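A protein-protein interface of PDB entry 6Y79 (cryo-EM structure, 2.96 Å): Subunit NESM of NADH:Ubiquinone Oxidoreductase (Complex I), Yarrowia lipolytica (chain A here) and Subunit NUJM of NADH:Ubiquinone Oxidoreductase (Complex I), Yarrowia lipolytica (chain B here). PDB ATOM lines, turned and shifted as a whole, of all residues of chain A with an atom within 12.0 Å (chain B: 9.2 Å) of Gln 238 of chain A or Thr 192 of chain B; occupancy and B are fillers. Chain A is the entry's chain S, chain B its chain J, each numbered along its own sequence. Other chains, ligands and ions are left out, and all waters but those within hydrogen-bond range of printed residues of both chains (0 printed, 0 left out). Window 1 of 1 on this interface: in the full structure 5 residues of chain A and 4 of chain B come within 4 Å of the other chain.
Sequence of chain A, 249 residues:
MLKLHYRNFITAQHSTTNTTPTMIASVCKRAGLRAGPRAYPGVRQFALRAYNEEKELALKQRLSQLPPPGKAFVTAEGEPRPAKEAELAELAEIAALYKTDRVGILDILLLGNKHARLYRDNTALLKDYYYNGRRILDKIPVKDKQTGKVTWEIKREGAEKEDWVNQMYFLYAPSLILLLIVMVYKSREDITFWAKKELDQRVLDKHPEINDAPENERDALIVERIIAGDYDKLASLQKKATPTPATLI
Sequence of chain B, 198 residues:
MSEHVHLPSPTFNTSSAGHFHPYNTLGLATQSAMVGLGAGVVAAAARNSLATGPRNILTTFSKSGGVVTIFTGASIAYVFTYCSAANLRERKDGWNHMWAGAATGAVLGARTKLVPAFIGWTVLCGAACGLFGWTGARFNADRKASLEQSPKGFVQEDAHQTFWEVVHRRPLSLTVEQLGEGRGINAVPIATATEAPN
Hydrophobic or aromatic side chains of chain B that line the printed part of chain A: Pro 189 and Ala 191.
Of the 12 printed residues of chain A, 5 touch a printed residue of chain B.
Hydrophobic or aromatic side chains of chain A that line the printed part of chain B: Leu 234 and Ala 235.
Among the printed residues, no Asp or Glu carboxylate lies within 4 Å of a Lys or Arg side-chain nitrogen of the other chain.
Among the printed residues, merely in contact across the chains: Leu 234 of chain A with Ala 191 of chain B (3.7 Å), Ala 235 of chain A with Glu 195 of chain B (3.8 Å), Gln 238 of chain A with Pro 189 of chain B (3.3 Å), Gln 238 of chain A with Ala 191 of chain B (3.5 Å), Gln 238 of chain A with Thr 192 of chain B (3.4 Å) and Thr 242 of chain A with Thr 192 of chain B (3.7 Å).
Gln 238 of chain A touches just these residues of chain B: Pro 189 (3.3 Å), Ala 191 (3.5 Å) and Thr 192 (3.4 Å).
Thr 192 of chain B touches two residues of chain A.
No residue of chain B comes within 4 Å of Ala 241 of chain A.
No residue of chain A comes within 4 Å of Val 188 of chain B.
Of chain A, only Gln 238 comes within 4 Å of Pro 189 of chain B.
No residue of chain A comes within 4 Å of Ile 190 of chain B.
Ala 191 of chain B touches just these residues of chain A: Leu 234 (3.7 Å) and Gln 238 (3.5 Å).
No residue of chain A comes within 4 Å of Ala 193 of chain B.
Printed residues of chain B within 4 Å of Asp 230 of chain A: Glu 195.
Of the printed residues of chain B, Thr 242 of chain A touches Thr 192 (3.7 Å).
Of the printed residues of chain B, Leu 234 of chain A touches Ala 191.
Lys 233 of chain A touches none of the printed residues of chain B.
Ala 196 of chain B touches none of the printed residues of chain A.
The nearest residue of chain B that does not touch Gln 238 of chain A is Ile 190 of chain B (5.5 Å).
The side-chain carboxylate of Asp 230 of chain A sits close to the side-chain carboxylate of Glu 195 of chain B.
The backbone carbonyl oxygen of Ala 191 of chain B sits close to the side-chain hydroxyl of Thr 194 of chain B, at 3.2 Å.
The backbone carbonyl oxygen (O) of Gln 238 of chain A lies within hydrogen-bond range of the side-chain hydroxyl (OG1) of Thr 242 of chain A (3.5 Å).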
ATOM      1  N   ASP A 230      21.088 -26.050  22.986  1.00  0.00           N
ATOM      2  CA  ASP A 230      20.998 -25.640  21.588  1.00  0.00           C
ATOM      3  C   ASP A 230      22.172 -26.151  20.762  1.00  0.00           C
ATOM      4  O   ASP A 230      21.969 -26.902  19.803  1.00  0.00           O
ATOM      5  CB  ASP A 230      20.950 -24.119  21.491  1.00  0.00           C
ATOM      6  CG  ASP A 230      19.709 -23.529  22.104  1.00  0.00           C
ATOM      7  OD1 ASP A 230      18.813 -24.287  22.533  1.00  0.00           O
ATOM      8  OD2 ASP A 230      19.635 -22.288  22.146  1.00  0.00           O
ATOM      9  N   ASP A 232      23.889 -24.643  18.560  1.00  0.00           N
ATOM     10  CA  ASP A 232      23.965 -24.168  17.178  1.00  0.00           C
ATOM     11  C   ASP A 232      25.097 -23.169  17.004  1.00  0.00           C
ATOM     12  O   ASP A 232      26.153 -23.523  16.473  1.00  0.00           O
ATOM     13  CB  ASP A 232      22.636 -23.543  16.753  1.00  0.00           C
ATOM     14  CG  ASP A 232      21.549 -24.572  16.641  1.00  0.00           C
ATOM     15  OD1 ASP A 232      21.838 -25.739  16.940  1.00  0.00           O
ATOM     16  OD2 ASP A 232      20.451 -24.192  16.240  1.00  0.00           O
ATOM     17  N   LYS A 233      24.940 -22.001  17.650  1.00  0.00           N
ATOM     18  CA  LYS A 233      25.509 -20.674  17.343  1.00  0.00           C
ATOM     19  C   LYS A 233      24.825 -19.987  16.164  1.00  0.00           C
ATOM     20  O   LYS A 233      25.503 -19.319  15.380  1.00  0.00           O
ATOM     21  CB  LYS A 233      27.025 -20.640  17.086  1.00  0.00           C
ATOM     22  CG  LYS A 233      27.877 -21.294  18.149  1.00  0.00           C
ATOM     23  CD  LYS A 233      29.258 -21.510  17.581  1.00  0.00           C
ATOM     24  CE  LYS A 233      30.064 -22.508  18.377  1.00  0.00           C
ATOM     25  NZ  LYS A 233      31.489 -22.451  17.947  1.00  0.00           N
ATOM     26  N   LEU A 234      23.511 -20.153  15.969  1.00  0.00           N
ATOM     27  CA  LEU A 234      22.822 -19.384  14.933  1.00  0.00           C
ATOM     28  C   LEU A 234      22.530 -17.959  15.389  1.00  0.00           C
ATOM     29  O   LEU A 234      22.677 -17.015  14.608  1.00  0.00           O
ATOM     30  CB  LEU A 234      21.526 -20.075  14.513  1.00  0.00           C
ATOM     31  CG  LEU A 234      20.876 -19.505  13.249  1.00  0.00           C
ATOM     32  CD1 LEU A 234      21.877 -19.345  12.124  1.00  0.00           C
ATOM     33  CD2 LEU A 234      19.753 -20.392  12.787  1.00  0.00           C
ATOM     34  N   ALA A 235      22.101 -17.776  16.642  1.00  0.00           N
ATOM     35  CA  ALA A 235      21.950 -16.424  17.181  1.00  0.00           C
ATOM     36  C   ALA A 235      23.291 -15.730  17.366  1.00  0.00           C
ATOM     37  O   ALA A 235      23.332 -14.491  17.449  1.00  0.00           O
ATOM     38  CB  ALA A 235      21.201 -16.466  18.510  1.00  0.00           C
ATOM     39  N   SER A 236      24.378 -16.511  17.455  1.00  0.00           N
ATOM     40  CA  SER A 236      25.705 -15.931  17.342  1.00  0.00           C
ATOM     41  C   SER A 236      25.911 -15.240  15.989  1.00  0.00           C
ATOM     42  O   SER A 236      26.578 -14.203  15.917  1.00  0.00           O
ATOM     43  CB  SER A 236      26.759 -16.996  17.567  1.00  0.00           C
ATOM     44  OG  SER A 236      27.984 -16.621  17.025  1.00  0.00           O
ATOM     45  N   LEU A 237      25.370 -15.794  14.903  1.00  0.00           N
ATOM     46  CA  LEU A 237      25.610 -15.216  13.580  1.00  0.00           C
ATOM     47  C   LEU A 237      24.774 -13.963  13.358  1.00  0.00           C
ATOM     48  O   LEU A 237      25.213 -13.035  12.676  1.00  0.00           O
ATOM     49  CB  LEU A 237      25.320 -16.244  12.495  1.00  0.00           C
ATOM     50  CG  LEU A 237      26.173 -17.504  12.537  1.00  0.00           C
ATOM     51  CD1 LEU A 237      25.743 -18.432  11.428  1.00  0.00           C
ATOM     52  CD2 LEU A 237      27.648 -17.191  12.431  1.00  0.00           C
ATOM     53  N   GLN A 238      23.569 -13.923  13.907  1.00  0.00           N
ATOM     54  CA  GLN A 238      22.665 -12.792  13.723  1.00  0.00           C
ATOM     55  C   GLN A 238      22.879 -11.724  14.790  1.00  0.00           C
ATOM     56  O   GLN A 238      21.982 -11.397  15.563  1.00  0.00           O
ATOM     57  CB  GLN A 238      21.230 -13.294  13.721  1.00  0.00           C
ATOM     58  CG  GLN A 238      21.058 -14.559  12.905  1.00  0.00           C
ATOM     59  CD  GLN A 238      19.611 -14.938  12.715  1.00  0.00           C
ATOM     60  OE1 GLN A 238      18.725 -14.407  13.379  1.00  0.00           O
ATOM     61  NE2 GLN A 238      19.361 -15.852  11.793  1.00  0.00           N
ATOM     62  N   LYS A 239      24.096 -11.174  14.826  1.00  0.00           N
ATOM     63  CA  LYS A 239      24.428 -10.156  15.814  1.00  0.00           C
ATOM     64  C   LYS A 239      23.724  -8.843  15.510  1.00  0.00           C
ATOM     65  O   LYS A 239      23.357  -8.099  16.426  1.00  0.00           O
ATOM     66  CB  LYS A 239      25.940  -9.957  15.863  1.00  0.00           C
ATOM     67  CG  LYS A 239      26.600 -10.056  14.511  1.00  0.00           C
ATOM     68  CD  LYS A 239      28.106 -10.003  14.622  1.00  0.00           C
ATOM     69  CE  LYS A 239      28.649 -11.242  15.302  1.00  0.00           C
ATOM     70  NZ  LYS A 239      28.259 -12.487  14.594  1.00  0.00           N
ATOM     71  N   LYS A 240      23.527  -8.542  14.227  1.00  0.00           N
ATOM     72  CA  LYS A 240      22.806  -7.332  13.844  1.00  0.00           C
ATOM     73  C   LYS A 240      21.327  -7.449  14.186  1.00  0.00           C
ATOM     74  O   LYS A 240      20.644  -6.441  14.390  1.00  0.00           O
ATOM     75  CB  LYS A 240      23.004  -7.069  12.351  1.00  0.00           C
ATOM     76  CG  LYS A 240      22.544  -5.712  11.844  1.00  0.00           C
ATOM     77  CD  LYS A 240      23.700  -4.734  11.761  1.00  0.00           C
ATOM     78  CE  LYS A 240      24.644  -5.081  10.628  1.00  0.00           C
ATOM     79  NZ  LYS A 240      25.841  -4.200  10.618  1.00  0.00           N
ATOM     80  N   ALA A 241      20.816  -8.678  14.255  1.00  0.00           N
ATOM     81  CA  ALA A 241      19.433  -8.885  14.667  1.00  0.00           C
ATOM     82  C   ALA A 241      19.263  -8.638  16.158  1.00  0.00           C
ATOM     83  O   ALA A 241      18.241  -8.095  16.592  1.00  0.00           O
ATOM     84  CB  ALA A 241      18.985 -10.299  14.302  1.00  0.00           C
ATOM     85  N   THR A 242      20.257  -9.017  16.952  1.00  0.00           N
ATOM     86  CA  THR A 242      20.186  -8.895  18.402  1.00  0.00           C
ATOM     87  C   THR A 242      20.801  -7.579  18.877  1.00  0.00           C
ATOM     88  O   THR A 242      22.022  -7.421  18.909  1.00  0.00           O
ATOM     89  CB  THR A 242      20.899 -10.075  19.093  1.00  0.00           C
ATOM     90  OG1 THR A 242      20.339 -11.307  18.625  1.00  0.00           O
ATOM     91  CG2 THR A 242      20.724 -10.002  20.601  1.00  0.00           C
ATOM     92  N   ARG B 169      21.900  -4.326   1.209  1.00  0.00           N
ATOM     93  CA  ARG B 169      20.868  -4.772   2.128  1.00  0.00           C
ATOM     94  C   ARG B 169      19.761  -3.738   2.173  1.00  0.00           C
ATOM     95  O   ARG B 169      20.024  -2.535   2.206  1.00  0.00           O
ATOM     96  CB  ARG B 169      21.406  -4.974   3.537  1.00  0.00           C
ATOM     97  CG  ARG B 169      22.361  -6.121   3.690  1.00  0.00           C
ATOM     98  CD  ARG B 169      22.977  -6.109   5.066  1.00  0.00           C
ATOM     99  NE  ARG B 169      22.051  -6.604   6.072  1.00  0.00           N
ATOM    100  CZ  ARG B 169      22.035  -7.858   6.498  1.00  0.00           C
ATOM    101  NH1 ARG B 169      22.896  -8.724   6.002  1.00  0.00           N
ATOM    102  NH2 ARG B 169      21.160  -8.248   7.411  1.00  0.00           N
ATOM    103  N   LEU B 172      14.518  -4.401   6.821  1.00  0.00           N
ATOM    104  CA  LEU B 172      13.562  -5.481   7.065  1.00  0.00           C
ATOM    105  C   LEU B 172      12.162  -4.950   7.334  1.00  0.00           C
ATOM    106  O   LEU B 172      11.174  -5.655   7.095  1.00  0.00           O
ATOM    107  CB  LEU B 172      14.027  -6.346   8.237  1.00  0.00           C
ATOM    108  CG  LEU B 172      13.475  -7.758   8.444  1.00  0.00           C
ATOM    109  CD1 LEU B 172      14.566  -8.661   8.967  1.00  0.00           C
ATOM    110  CD2 LEU B 172      12.321  -7.758   9.415  1.00  0.00           C
ATOM    111  N   ALA B 187       8.843 -10.327  11.181  1.00  0.00           N
ATOM    112  CA  ALA B 187       9.485  -9.090  11.601  1.00  0.00           C
ATOM    113  C   ALA B 187      10.769  -9.322  12.381  1.00  0.00           C
ATOM    114  O   ALA B 187      11.549  -8.382  12.556  1.00  0.00           O
ATOM    115  CB  ALA B 187       8.516  -8.262  12.445  1.00  0.00           C
ATOM    116  N   VAL B 188      10.983 -10.527  12.895  1.00  0.00           N
ATOM    117  CA  VAL B 188      12.224 -10.929  13.552  1.00  0.00           C
ATOM    118  C   VAL B 188      12.533 -12.296  12.956  1.00  0.00           C
ATOM    119  O   VAL B 188      11.593 -13.057  12.691  1.00  0.00           O
ATOM    120  CB  VAL B 188      12.078 -10.981  15.088  1.00  0.00           C
ATOM    121  CG1 VAL B 188      13.357 -11.456  15.755  1.00  0.00           C
ATOM    122  CG2 VAL B 188      11.695  -9.634  15.672  1.00  0.00           C
ATOM    123  N   PRO B 189      13.795 -12.630  12.671  1.00  0.00           N
ATOM    124  CA  PRO B 189      14.109 -13.969  12.157  1.00  0.00           C
ATOM    125  C   PRO B 189      13.748 -15.084  13.131  1.00  0.00           C
ATOM    126  O   PRO B 189      13.586 -14.864  14.333  1.00  0.00           O
ATOM    127  CB  PRO B 189      15.622 -13.908  11.911  1.00  0.00           C
ATOM    128  CG  PRO B 189      16.078 -12.587  12.442  1.00  0.00           C
ATOM    129  CD  PRO B 189      14.900 -11.694  12.425  1.00  0.00           C
ATOM    130  N   ILE B 190      13.595 -16.288  12.570  1.00  0.00           N
ATOM    131  CA  ILE B 190      13.144 -17.468  13.307  1.00  0.00           C
ATOM    132  C   ILE B 190      14.148 -17.853  14.383  1.00  0.00           C
ATOM    133  O   ILE B 190      13.771 -18.352  15.451  1.00  0.00           O
ATOM    134  CB  ILE B 190      12.892 -18.620  12.307  1.00  0.00           C
ATOM    135  CG1 ILE B 190      11.832 -18.205  11.293  1.00  0.00           C
ATOM    136  CG2 ILE B 190      12.422 -19.895  12.996  1.00  0.00           C
ATOM    137  CD1 ILE B 190      10.479 -17.954  11.924  1.00  0.00           C
ATOM    138  N   ALA B 191      15.428 -17.593  14.136  1.00  0.00           N
ATOM    139  CA  ALA B 191      16.502 -17.919  15.061  1.00  0.00           C
ATOM    140  C   ALA B 191      16.393 -17.161  16.374  1.00  0.00           C
ATOM    141  O   ALA B 191      16.251 -17.775  17.432  1.00  0.00           O
ATOM    142  CB  ALA B 191      17.852 -17.623  14.417  1.00  0.00           C
ATOM    143  N   THR B 192      16.444 -15.833  16.323  1.00  0.00           N
ATOM    144  CA  THR B 192      16.470 -15.052  17.551  1.00  0.00           C
ATOM    145  C   THR B 192      15.104 -14.916  18.203  1.00  0.00           C
ATOM    146  O   THR B 192      15.030 -14.459  19.348  1.00  0.00           O
ATOM    147  CB  THR B 192      17.051 -13.669  17.281  1.00  0.00           C
ATOM    148  OG1 THR B 192      16.229 -12.990  16.329  1.00  0.00           O
ATOM    149  CG2 THR B 192      18.452 -13.793  16.726  1.00  0.00           C
ATOM    150  N   ALA B 193      14.027 -15.294  17.516  1.00  0.00           N
ATOM    151  CA  ALA B 193      12.748 -15.425  18.200  1.00  0.00           C
ATOM    152  C   ALA B 193      12.736 -16.644  19.112  1.00  0.00           C
ATOM    153  O   ALA B 193      11.991 -16.673  20.096  1.00  0.00           O
ATOM    154  CB  ALA B 193      11.612 -15.499  17.181  1.00  0.00           C
ATOM    155  N   THR B 194      13.539 -17.657  18.801  1.00  0.00           N
ATOM    156  CA  THR B 194      13.694 -18.848  19.631  1.00  0.00           C
ATOM    157  C   THR B 194      15.128 -18.916  20.146  1.00  0.00           C
ATOM    158  O   THR B 194      15.967 -19.621  19.590  1.00  0.00           O
ATOM    159  CB  THR B 194      13.372 -20.108  18.830  1.00  0.00           C
ATOM    160  OG1 THR B 194      14.416 -20.330  17.873  1.00  0.00           O
ATOM    161  CG2 THR B 194      12.049 -19.975  18.103  1.00  0.00           C
ATOM    162  N   GLU B 195      15.402 -18.212  21.239  1.00  0.00           N
ATOM    163  CA  GLU B 195      16.701 -18.311  21.881  1.00  0.00           C
ATOM    164  C   GLU B 195      16.545 -18.385  23.398  1.00  0.00           C
ATOM    165  O   GLU B 195      15.655 -17.764  23.986  1.00  0.00           O
ATOM    166  CB  GLU B 195      17.621 -17.150  21.445  1.00  0.00           C
ATOM    167  CG  GLU B 195      19.078 -17.264  21.910  1.00  0.00           C
ATOM    168  CD  GLU B 195      19.762 -18.578  21.502  1.00  0.00           C
ATOM    169  OE1 GLU B 195      19.433 -19.165  20.447  1.00  0.00           O
ATOM    170  OE2 GLU B 195      20.620 -19.050  22.278  1.00  0.00           O
ATOM    171  N   ALA B 196      17.454 -19.153  24.020  1.00  0.00           N
ATOM    172  CA  ALA B 196      17.438 -19.713  25.370  1.00  0.00           C
ATOM    173  C   ALA B 196      17.174 -18.740  26.523  1.00  0.00           C
ATOM    174  O   ALA B 196      16.508 -19.140  27.488  1.00  0.00           O
ATOM    175  CB  ALA B 196      18.763 -20.450  25.608  1.00  0.00           C
ATOM    176  N   PRO B 197      17.684 -17.486  26.513  1.00  0.00           N
ATOM    177  CA  PRO B 197      17.132 -16.678  27.605  1.00  0.00           C
ATOM    178  C   PRO B 197      15.877 -15.922  27.179  1.00  0.00           C
ATOM    179  O   PRO B 197      14.854 -16.563  26.935  1.00  0.00           O
ATOM    180  CB  PRO B 197      18.271 -15.717  27.938  1.00  0.00           C
ATOM    181  CG  PRO B 197      18.942 -15.510  26.640  1.00  0.00           C
ATOM    182  CD  PRO B 197      18.851 -16.822  25.897  1.00  0.00           C
